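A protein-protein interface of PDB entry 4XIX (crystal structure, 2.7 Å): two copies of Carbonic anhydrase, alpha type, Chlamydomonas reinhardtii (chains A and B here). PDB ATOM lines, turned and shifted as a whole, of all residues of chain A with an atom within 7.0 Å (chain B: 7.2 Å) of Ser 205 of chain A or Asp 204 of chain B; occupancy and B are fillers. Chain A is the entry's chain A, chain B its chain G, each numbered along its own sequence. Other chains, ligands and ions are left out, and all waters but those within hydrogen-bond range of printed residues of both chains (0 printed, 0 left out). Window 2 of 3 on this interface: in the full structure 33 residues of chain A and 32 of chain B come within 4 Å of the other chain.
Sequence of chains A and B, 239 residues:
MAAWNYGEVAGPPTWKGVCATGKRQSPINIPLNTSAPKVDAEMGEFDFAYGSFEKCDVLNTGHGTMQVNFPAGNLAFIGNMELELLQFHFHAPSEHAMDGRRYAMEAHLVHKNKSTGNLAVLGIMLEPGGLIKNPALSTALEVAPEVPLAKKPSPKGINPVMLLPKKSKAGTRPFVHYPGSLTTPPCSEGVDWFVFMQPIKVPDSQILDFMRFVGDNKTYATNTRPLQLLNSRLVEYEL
Of the 13 printed residues of chain B, 4 touch a printed residue of chain A. Hydrophobic or aromatic side chains of chain B within 4 Å of the printed part of chain A: Pro 128 and Leu 208. Along chain B the printed residues that touch a printed residue of chain A span positions 128 to 208. Among the printed residues, no Asp or Glu carboxylate lies within 4 Å of a Lys or Arg side-chain nitrogen of the other chain.
Among the printed residues, pairs that only touch across the chains: Asp 204 of chain A with Asp 204 of chain B (3.5 Å), Asp 204 of chain A with Ser 205 of chain B (3.3 Å), Asp 204 of chain A with Leu 208 of chain B (3.9 Å), Ser 205 of chain A with Asp 204 of chain B (3.2 Å), Ile 207 of chain A with Leu 208 of chain B (3.8 Å), Leu 208 of chain A with Pro 128 of chain B (3.8 Å), Leu 208 of chain A with Asp 204 of chain B (3.8 Å) and Leu 208 of chain A with Leu 208 of chain B (3.7 Å).
The side-chain carboxylate of Asp 204 of chain B is in hydrogen-bond range of the backbone NH of Gly 129 of chain B (3.2 Å).
Asp 204 of chain B touches its own counterpart, Asp 204 of chain A. Asp 204 of chain A touches Ser 205 of chain B, and with the chains exchanged Ser 205 of chain A touches Asp 204 of chain B. Asp 204 of chain A touches Leu 208 of chain B, and with the chains exchanged Leu 208 of chain A touches Asp 204 of chain B. Ile 207 of chain A touches Leu 208 of chain B, but with the chains exchanged Leu 208 of chain A does not touch Ile 207 of chain B (4.1 Å). Of the 8 pairs that touch across the chains among the printed residues, 6 have their exchanged pair printed and touching as well.
Of the printed residues of chain B, Asp 204 of chain A touches Asp 204 (3.5 Å), Ser 205 (3.3 Å) and Leu 208 (3.9 Å). Ser 205 of chain A touches just one residue of chain B: Asp 204. Printed residues of chain B within 4 Å of Ile 207 of chain A: Leu 208 (3.8 Å). Of the printed residues of chain B, Leu 208 of chain A touches Pro 128 (3.8 Å), Asp 204 (3.8 Å) and Leu 208 (3.7 Å). Of chain A, only Asp 204 (3.5 Å), Ser 205 (3.2 Å) and Leu 208 (3.8 Å) come within 4 Å of Asp 204 of chain B. Printed residues of chain A within 4 Å of Ser 205 of chain B: Asp 204. Printed residues of chain A within 4 Å of Leu 208 of chain B: Asp 204, Ile 207 and Leu 208. The nearest printed residue of chain A that does not touch Ser 205 of chain B is Leu 208 of chain A (6.1 Å).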
ATOM      1  N   GLY A 130      13.174  -2.151 -10.201  1.00  0.00           N
ATOM      2  CA  GLY A 130      14.163  -3.008 -10.805  1.00  0.00           C
ATOM      3  C   GLY A 130      15.021  -2.296 -11.836  1.00  0.00           C
ATOM      4  O   GLY A 130      14.598  -1.314 -12.456  1.00  0.00           O
ATOM      5  N   LYS A 133      15.758  -5.939 -16.761  1.00  0.00           N
ATOM      6  CA  LYS A 133      14.520  -6.235 -17.449  1.00  0.00           C
ATOM      7  C   LYS A 133      14.239  -7.668 -17.234  1.00  0.00           C
ATOM      8  O   LYS A 133      15.107  -8.507 -17.451  1.00  0.00           O
ATOM      9  CB  LYS A 133      14.609  -5.947 -18.943  1.00  0.00           C
ATOM     10  CG  LYS A 133      14.304  -4.465 -19.302  1.00  0.00           C
ATOM     11  CD  LYS A 133      13.365  -4.323 -20.508  1.00  0.00           C
ATOM     12  CE  LYS A 133      13.897  -5.077 -21.755  1.00  0.00           C
ATOM     13  NZ  LYS A 133      12.967  -5.038 -22.935  1.00  0.00           N
ATOM     14  N   LEU A 141       5.637  -9.331 -23.760  1.00  0.00           N
ATOM     15  CA  LEU A 141       5.221  -8.074 -24.391  1.00  0.00           C
ATOM     16  C   LEU A 141       5.607  -7.968 -25.886  1.00  0.00           C
ATOM     17  O   LEU A 141       4.803  -7.537 -26.702  1.00  0.00           O
ATOM     18  CB  LEU A 141       5.859  -6.917 -23.652  1.00  0.00           C
ATOM     19  CG  LEU A 141       5.381  -6.744 -22.239  1.00  0.00           C
ATOM     20  CD1 LEU A 141       6.345  -5.849 -21.460  1.00  0.00           C
ATOM     21  CD2 LEU A 141       4.012  -6.134 -22.336  1.00  0.00           C
ATOM     22  N   VAL A 202      10.866  -5.444 -10.979  1.00  0.00           N
ATOM     23  CA  VAL A 202      10.880  -5.326 -12.410  1.00  0.00           C
ATOM     24  C   VAL A 202      11.231  -3.874 -12.620  1.00  0.00           C
ATOM     25  O   VAL A 202      11.108  -3.096 -11.689  1.00  0.00           O
ATOM     26  CB  VAL A 202       9.491  -5.670 -12.892  1.00  0.00           C
ATOM     27  CG1 VAL A 202       9.098  -4.849 -14.030  1.00  0.00           C
ATOM     28  CG2 VAL A 202       9.422  -7.149 -13.248  1.00  0.00           C
ATOM     29  N   PRO A 203      11.717  -3.496 -13.811  1.00  0.00           N
ATOM     30  CA  PRO A 203      11.889  -2.058 -14.101  1.00  0.00           C
ATOM     31  C   PRO A 203      10.586  -1.334 -14.444  1.00  0.00           C
ATOM     32  O   PRO A 203       9.704  -1.890 -15.103  1.00  0.00           O
ATOM     33  CB  PRO A 203      12.795  -2.053 -15.330  1.00  0.00           C
ATOM     34  CG  PRO A 203      13.379  -3.440 -15.390  1.00  0.00           C
ATOM     35  CD  PRO A 203      12.350  -4.334 -14.836  1.00  0.00           C
ATOM     36  N   ASP A 204      10.493  -0.074 -14.019  1.00  0.00           N
ATOM     37  CA  ASP A 204       9.313   0.796 -14.267  1.00  0.00           C
ATOM     38  C   ASP A 204       8.860   0.871 -15.697  1.00  0.00           C
ATOM     39  O   ASP A 204       7.672   0.843 -15.976  1.00  0.00           O
ATOM     40  CB  ASP A 204       9.616   2.192 -13.799  1.00  0.00           C
ATOM     41  CG  ASP A 204      10.108   2.207 -12.370  1.00  0.00           C
ATOM     42  OD1 ASP A 204      10.956   1.332 -12.025  1.00  0.00           O
ATOM     43  OD2 ASP A 204       9.613   3.055 -11.590  1.00  0.00           O
ATOM     44  N   SER A 205       9.813   0.934 -16.609  1.00  0.00           N
ATOM     45  CA  SER A 205       9.498   0.838 -18.014  1.00  0.00           C
ATOM     46  C   SER A 205       8.640  -0.394 -18.295  1.00  0.00           C
ATOM     47  O   SER A 205       7.642  -0.286 -18.982  1.00  0.00           O
ATOM     48  CB  SER A 205      10.778   0.804 -18.831  1.00  0.00           C
ATOM     49  OG  SER A 205      11.459  -0.431 -18.648  1.00  0.00           O
ATOM     50  N   GLN A 206       8.982  -1.560 -17.754  1.00  0.00           N
ATOM     51  CA  GLN A 206       8.201  -2.726 -18.106  1.00  0.00           C
ATOM     52  C   GLN A 206       6.781  -2.644 -17.556  1.00  0.00           C
ATOM     53  O   GLN A 206       5.818  -3.024 -18.232  1.00  0.00           O
ATOM     54  CB  GLN A 206       8.877  -4.011 -17.642  1.00  0.00           C
ATOM     55  CG  GLN A 206      10.202  -4.242 -18.312  1.00  0.00           C
ATOM     56  CD  GLN A 206      10.703  -5.658 -18.159  1.00  0.00           C
ATOM     57  OE1 GLN A 206      11.124  -6.071 -17.075  1.00  0.00           O
ATOM     58  NE2 GLN A 206      10.670  -6.411 -19.261  1.00  0.00           N
ATOM     59  N   ILE A 207       6.625  -2.177 -16.328  1.00  0.00           N
ATOM     60  CA  ILE A 207       5.272  -2.001 -15.815  1.00  0.00           C
ATOM     61  C   ILE A 207       4.452  -1.062 -16.724  1.00  0.00           C
ATOM     62  O   ILE A 207       3.307  -1.386 -17.100  1.00  0.00           O
ATOM     63  CB  ILE A 207       5.293  -1.471 -14.396  1.00  0.00           C
ATOM     64  CG1 ILE A 207       5.757  -2.590 -13.473  1.00  0.00           C
ATOM     65  CG2 ILE A 207       3.916  -0.885 -13.959  1.00  0.00           C
ATOM     66  CD1 ILE A 207       6.449  -2.015 -12.211  1.00  0.00           C
ATOM     67  N   LEU A 208       5.016   0.086 -17.097  1.00  0.00           N
ATOM     68  CA  LEU A 208       4.276   0.978 -18.004  1.00  0.00           C
ATOM     69  C   LEU A 208       4.018   0.330 -19.356  1.00  0.00           C
ATOM     70  O   LEU A 208       2.947   0.478 -19.913  1.00  0.00           O
ATOM     71  CB  LEU A 208       4.984   2.308 -18.204  1.00  0.00           C
ATOM     72  CG  LEU A 208       4.999   3.188 -16.969  1.00  0.00           C
ATOM     73  CD1 LEU A 208       5.635   4.510 -17.331  1.00  0.00           C
ATOM     74  CD2 LEU A 208       3.621   3.395 -16.435  1.00  0.00           C
ATOM     75  N   ASP A 209       4.979  -0.419 -19.868  1.00  0.00           N
ATOM     76  CA  ASP A 209       4.760  -1.146 -21.099  1.00  0.00           C
ATOM     77  C   ASP A 209       3.528  -1.999 -20.982  1.00  0.00           C
ATOM     78  O   ASP A 209       2.756  -2.135 -21.933  1.00  0.00           O
ATOM     79  CB  ASP A 209       5.944  -2.063 -21.392  1.00  0.00           C
ATOM     80  CG  ASP A 209       7.090  -1.357 -22.099  1.00  0.00           C
ATOM     81  OD1 ASP A 209       7.163  -0.097 -22.037  1.00  0.00           O
ATOM     82  OD2 ASP A 209       7.920  -2.080 -22.726  1.00  0.00           O
ATOM     83  N   PHE A 210       3.374  -2.642 -19.832  1.00  0.00           N
ATOM     84  CA  PHE A 210       2.263  -3.558 -19.699  1.00  0.00           C
ATOM     85  C   PHE A 210       0.964  -2.783 -19.637  1.00  0.00           C
ATOM     86  O   PHE A 210       0.000  -3.103 -20.359  1.00  0.00           O
ATOM     87  CB  PHE A 210       2.410  -4.480 -18.497  1.00  0.00           C
ATOM     88  CG  PHE A 210       1.244  -5.396 -18.313  1.00  0.00           C
ATOM     89  CD1 PHE A 210       1.065  -6.478 -19.152  1.00  0.00           C
ATOM     90  CD2 PHE A 210       0.309  -5.160 -17.318  1.00  0.00           C
ATOM     91  CE1 PHE A 210      -0.008  -7.321 -19.010  1.00  0.00           C
ATOM     92  CE2 PHE A 210      -0.777  -6.014 -17.160  1.00  0.00           C
ATOM     93  CZ  PHE A 210      -0.934  -7.097 -18.015  1.00  0.00           C
ATOM     94  N   MET A 211       0.915  -1.767 -18.784  1.00  0.00           N
ATOM     95  CA  MET A 211      -0.289  -0.918 -18.737  1.00  0.00           C
ATOM     96  C   MET A 211      -0.618  -0.354 -20.131  1.00  0.00           C
ATOM     97  O   MET A 211      -1.773  -0.285 -20.520  1.00  0.00           O
ATOM     98  CB  MET A 211      -0.114   0.203 -17.733  1.00  0.00           C
ATOM     99  CG  MET A 211      -0.099  -0.269 -16.283  1.00  0.00           C
ATOM    100  SD  MET A 211       0.253   1.096 -15.141  1.00  0.00           S
ATOM    101  CE  MET A 211       0.001   0.345 -13.508  1.00  0.00           C
ATOM    102  N   GLU B 127       5.365  12.157 -21.268  1.00  0.00           N
ATOM    103  CA  GLU B 127       5.777  10.829 -21.711  1.00  0.00           C
ATOM    104  C   GLU B 127       6.772  10.168 -20.746  1.00  0.00           C
ATOM    105  O   GLU B 127       7.528  10.855 -20.078  1.00  0.00           O
ATOM    106  CB  GLU B 127       6.563  10.985 -22.986  1.00  0.00           C
ATOM    107  CG  GLU B 127       5.794  11.003 -24.248  1.00  0.00           C
ATOM    108  CD  GLU B 127       6.748  11.196 -25.413  1.00  0.00           C
ATOM    109  OE1 GLU B 127       7.815  11.841 -25.185  1.00  0.00           O
ATOM    110  OE2 GLU B 127       6.467  10.674 -26.523  1.00  0.00           O
ATOM    111  N   PRO B 128       6.852   8.827 -20.744  1.00  0.00           N
ATOM    112  CA  PRO B 128       7.933   8.181 -19.983  1.00  0.00           C
ATOM    113  C   PRO B 128       9.242   8.190 -20.782  1.00  0.00           C
ATOM    114  O   PRO B 128       9.209   8.487 -21.968  1.00  0.00           O
ATOM    115  CB  PRO B 128       7.419   6.768 -19.824  1.00  0.00           C
ATOM    116  CG  PRO B 128       6.637   6.527 -21.105  1.00  0.00           C
ATOM    117  CD  PRO B 128       6.082   7.855 -21.545  1.00  0.00           C
ATOM    118  N   GLY B 129      10.375   7.892 -20.154  1.00  0.00           N
ATOM    119  CA  GLY B 129      11.653   7.797 -20.869  1.00  0.00           C
ATOM    120  C   GLY B 129      12.586   8.989 -20.682  1.00  0.00           C
ATOM    121  O   GLY B 129      13.519   9.237 -21.462  1.00  0.00           O
ATOM    122  N   GLY B 130      12.347   9.727 -19.617  1.00  0.00           N
ATOM    123  CA  GLY B 130      13.128  10.904 -19.337  1.00  0.00           C
ATOM    124  C   GLY B 130      14.240  10.537 -18.410  1.00  0.00           C
ATOM    125  O   GLY B 130      14.065   9.688 -17.551  1.00  0.00           O
ATOM    126  N   VAL B 202       9.644  12.107 -19.078  1.00  0.00           N
ATOM    127  CA  VAL B 202       9.717  12.073 -17.628  1.00  0.00           C
ATOM    128  C   VAL B 202      10.157  10.672 -17.202  1.00  0.00           C
ATOM    129  O   VAL B 202       9.883   9.683 -17.888  1.00  0.00           O
ATOM    130  CB  VAL B 202       8.346  12.474 -17.035  1.00  0.00           C
ATOM    131  CG1 VAL B 202       8.224  12.142 -15.600  1.00  0.00           C
ATOM    132  CG2 VAL B 202       8.181  13.956 -17.149  1.00  0.00           C
ATOM    133  N   PRO B 203      10.868  10.568 -16.078  1.00  0.00           N
ATOM    134  CA  PRO B 203      11.278   9.223 -15.696  1.00  0.00           C
ATOM    135  C   PRO B 203      10.057   8.405 -15.284  1.00  0.00           C
ATOM    136  O   PRO B 203       9.182   8.911 -14.582  1.00  0.00           O
ATOM    137  CB  PRO B 203      12.197   9.473 -14.503  1.00  0.00           C
ATOM    138  CG  PRO B 203      12.577  10.820 -14.571  1.00  0.00           C
ATOM    139  CD  PRO B 203      11.402  11.559 -15.143  1.00  0.00           C
ATOM    140  N   ASP B 204      10.015   7.148 -15.710  1.00  0.00           N
ATOM    141  CA  ASP B 204       8.889   6.259 -15.439  1.00  0.00           C
ATOM    142  C   ASP B 204       8.577   6.192 -13.930  1.00  0.00           C
ATOM    143  O   ASP B 204       7.413   6.007 -13.517  1.00  0.00           O
ATOM    144  CB  ASP B 204       9.173   4.861 -16.010  1.00  0.00           C
ATOM    145  CG  ASP B 204       9.688   4.900 -17.461  1.00  0.00           C
ATOM    146  OD1 ASP B 204      10.500   5.786 -17.789  1.00  0.00           O
ATOM    147  OD2 ASP B 204       9.287   4.058 -18.293  1.00  0.00           O
ATOM    148  N   SER B 205       9.606   6.381 -13.113  1.00  0.00           N
ATOM    149  CA  SER B 205       9.417   6.375 -11.685  1.00  0.00           C
ATOM    150  C   SER B 205       8.333   7.357 -11.337  1.00  0.00           C
ATOM    151  O   SER B 205       7.456   7.034 -10.548  1.00  0.00           O
ATOM    152  CB  SER B 205      10.713   6.684 -10.934  1.00  0.00           C
ATOM    153  OG  SER B 205      10.928   8.061 -10.753  1.00  0.00           O
ATOM    154  N   GLN B 206       8.365   8.547 -11.944  1.00  0.00           N
ATOM    155  CA  GLN B 206       7.497   9.631 -11.502  1.00  0.00           C
ATOM    156  C   GLN B 206       6.071   9.381 -11.921  1.00  0.00           C
ATOM    157  O   GLN B 206       5.136   9.639 -11.162  1.00  0.00           O
ATOM    158  CB  GLN B 206       7.988  10.963 -12.035  1.00  0.00           C
ATOM    159  CG  GLN B 206       8.851  11.698 -11.037  1.00  0.00           C
ATOM    160  CD  GLN B 206       9.435  12.970 -11.603  1.00  0.00           C
ATOM    161  OE1 GLN B 206       9.645  13.092 -12.813  1.00  0.00           O
ATOM    162  NE2 GLN B 206       9.721  13.922 -10.725  1.00  0.00           N
ATOM    163  N   ILE B 207       5.903   8.864 -13.129  1.00  0.00           N
ATOM    164  CA  ILE B 207       4.580   8.473 -13.581  1.00  0.00           C
ATOM    165  C   ILE B 207       3.956   7.400 -12.641  1.00  0.00           C
ATOM    166  O   ILE B 207       2.786   7.568 -12.208  1.00  0.00           O
ATOM    167  CB  ILE B 207       4.630   8.001 -15.035  1.00  0.00           C
ATOM    168  CG1 ILE B 207       4.955   9.192 -15.928  1.00  0.00           C
ATOM    169  CG2 ILE B 207       3.317   7.398 -15.435  1.00  0.00           C
ATOM    170  CD1 ILE B 207       5.385   8.833 -17.339  1.00  0.00           C
ATOM    171  N   LEU B 208       4.716   6.339 -12.302  1.00  0.00           N
ATOM    172  CA  LEU B 208       4.179   5.347 -11.367  1.00  0.00           C
ATOM    173  C   LEU B 208       3.952   5.951  -9.993  1.00  0.00           C
ATOM    174  O   LEU B 208       2.963   5.631  -9.345  1.00  0.00           O
ATOM    175  CB  LEU B 208       5.060   4.107 -11.237  1.00  0.00           C
ATOM    176  CG  LEU B 208       5.048   3.112 -12.396  1.00  0.00           C
ATOM    177  CD1 LEU B 208       5.871   1.905 -12.018  1.00  0.00           C
ATOM    178  CD2 LEU B 208       3.631   2.700 -12.826  1.00  0.00           C
ATOM    179  N   ASP B 209       4.861   6.816  -9.544  1.00  0.00           N
ATOM    180  CA  ASP B 209       4.672   7.546  -8.286  1.00  0.00           C
ATOM    181  C   ASP B 209       3.361   8.347  -8.279  1.00  0.00           C
ATOM    182  O   ASP B 209       2.638   8.370  -7.286  1.00  0.00           O
ATOM    183  CB  ASP B 209       5.826   8.525  -8.030  1.00  0.00           C
ATOM    184  CG  ASP B 209       7.129   7.831  -7.664  1.00  0.00           C
ATOM    185  OD1 ASP B 209       7.089   6.663  -7.203  1.00  0.00           O
ATOM    186  OD2 ASP B 209       8.205   8.462  -7.838  1.00  0.00           O
ATOM    187  N   PHE B 210       3.055   9.027  -9.375  1.00  0.00           N
ATOM    188  CA  PHE B 210       1.810   9.775  -9.437  1.00  0.00           C
ATOM    189  C   PHE B 210       0.605   8.831  -9.438  1.00  0.00           C
ATOM    190  O   PHE B 210      -0.352   9.045  -8.684  1.00  0.00           O
ATOM    191  CB  PHE B 210       1.751  10.696 -10.663  1.00  0.00           C
ATOM    192  CG  PHE B 210       0.454  11.372 -10.794  1.00  0.00           C
ATOM    193  CD1 PHE B 210       0.124  12.424  -9.940  1.00  0.00           C
ATOM    194  CD2 PHE B 210      -0.486  10.915 -11.691  1.00  0.00           C
ATOM    195  CE1 PHE B 210      -1.084  13.037 -10.016  1.00  0.00           C
ATOM    196  CE2 PHE B 210      -1.724  11.527 -11.762  1.00  0.00           C
ATOM    197  CZ  PHE B 210      -2.011  12.593 -10.920  1.00  0.00           C
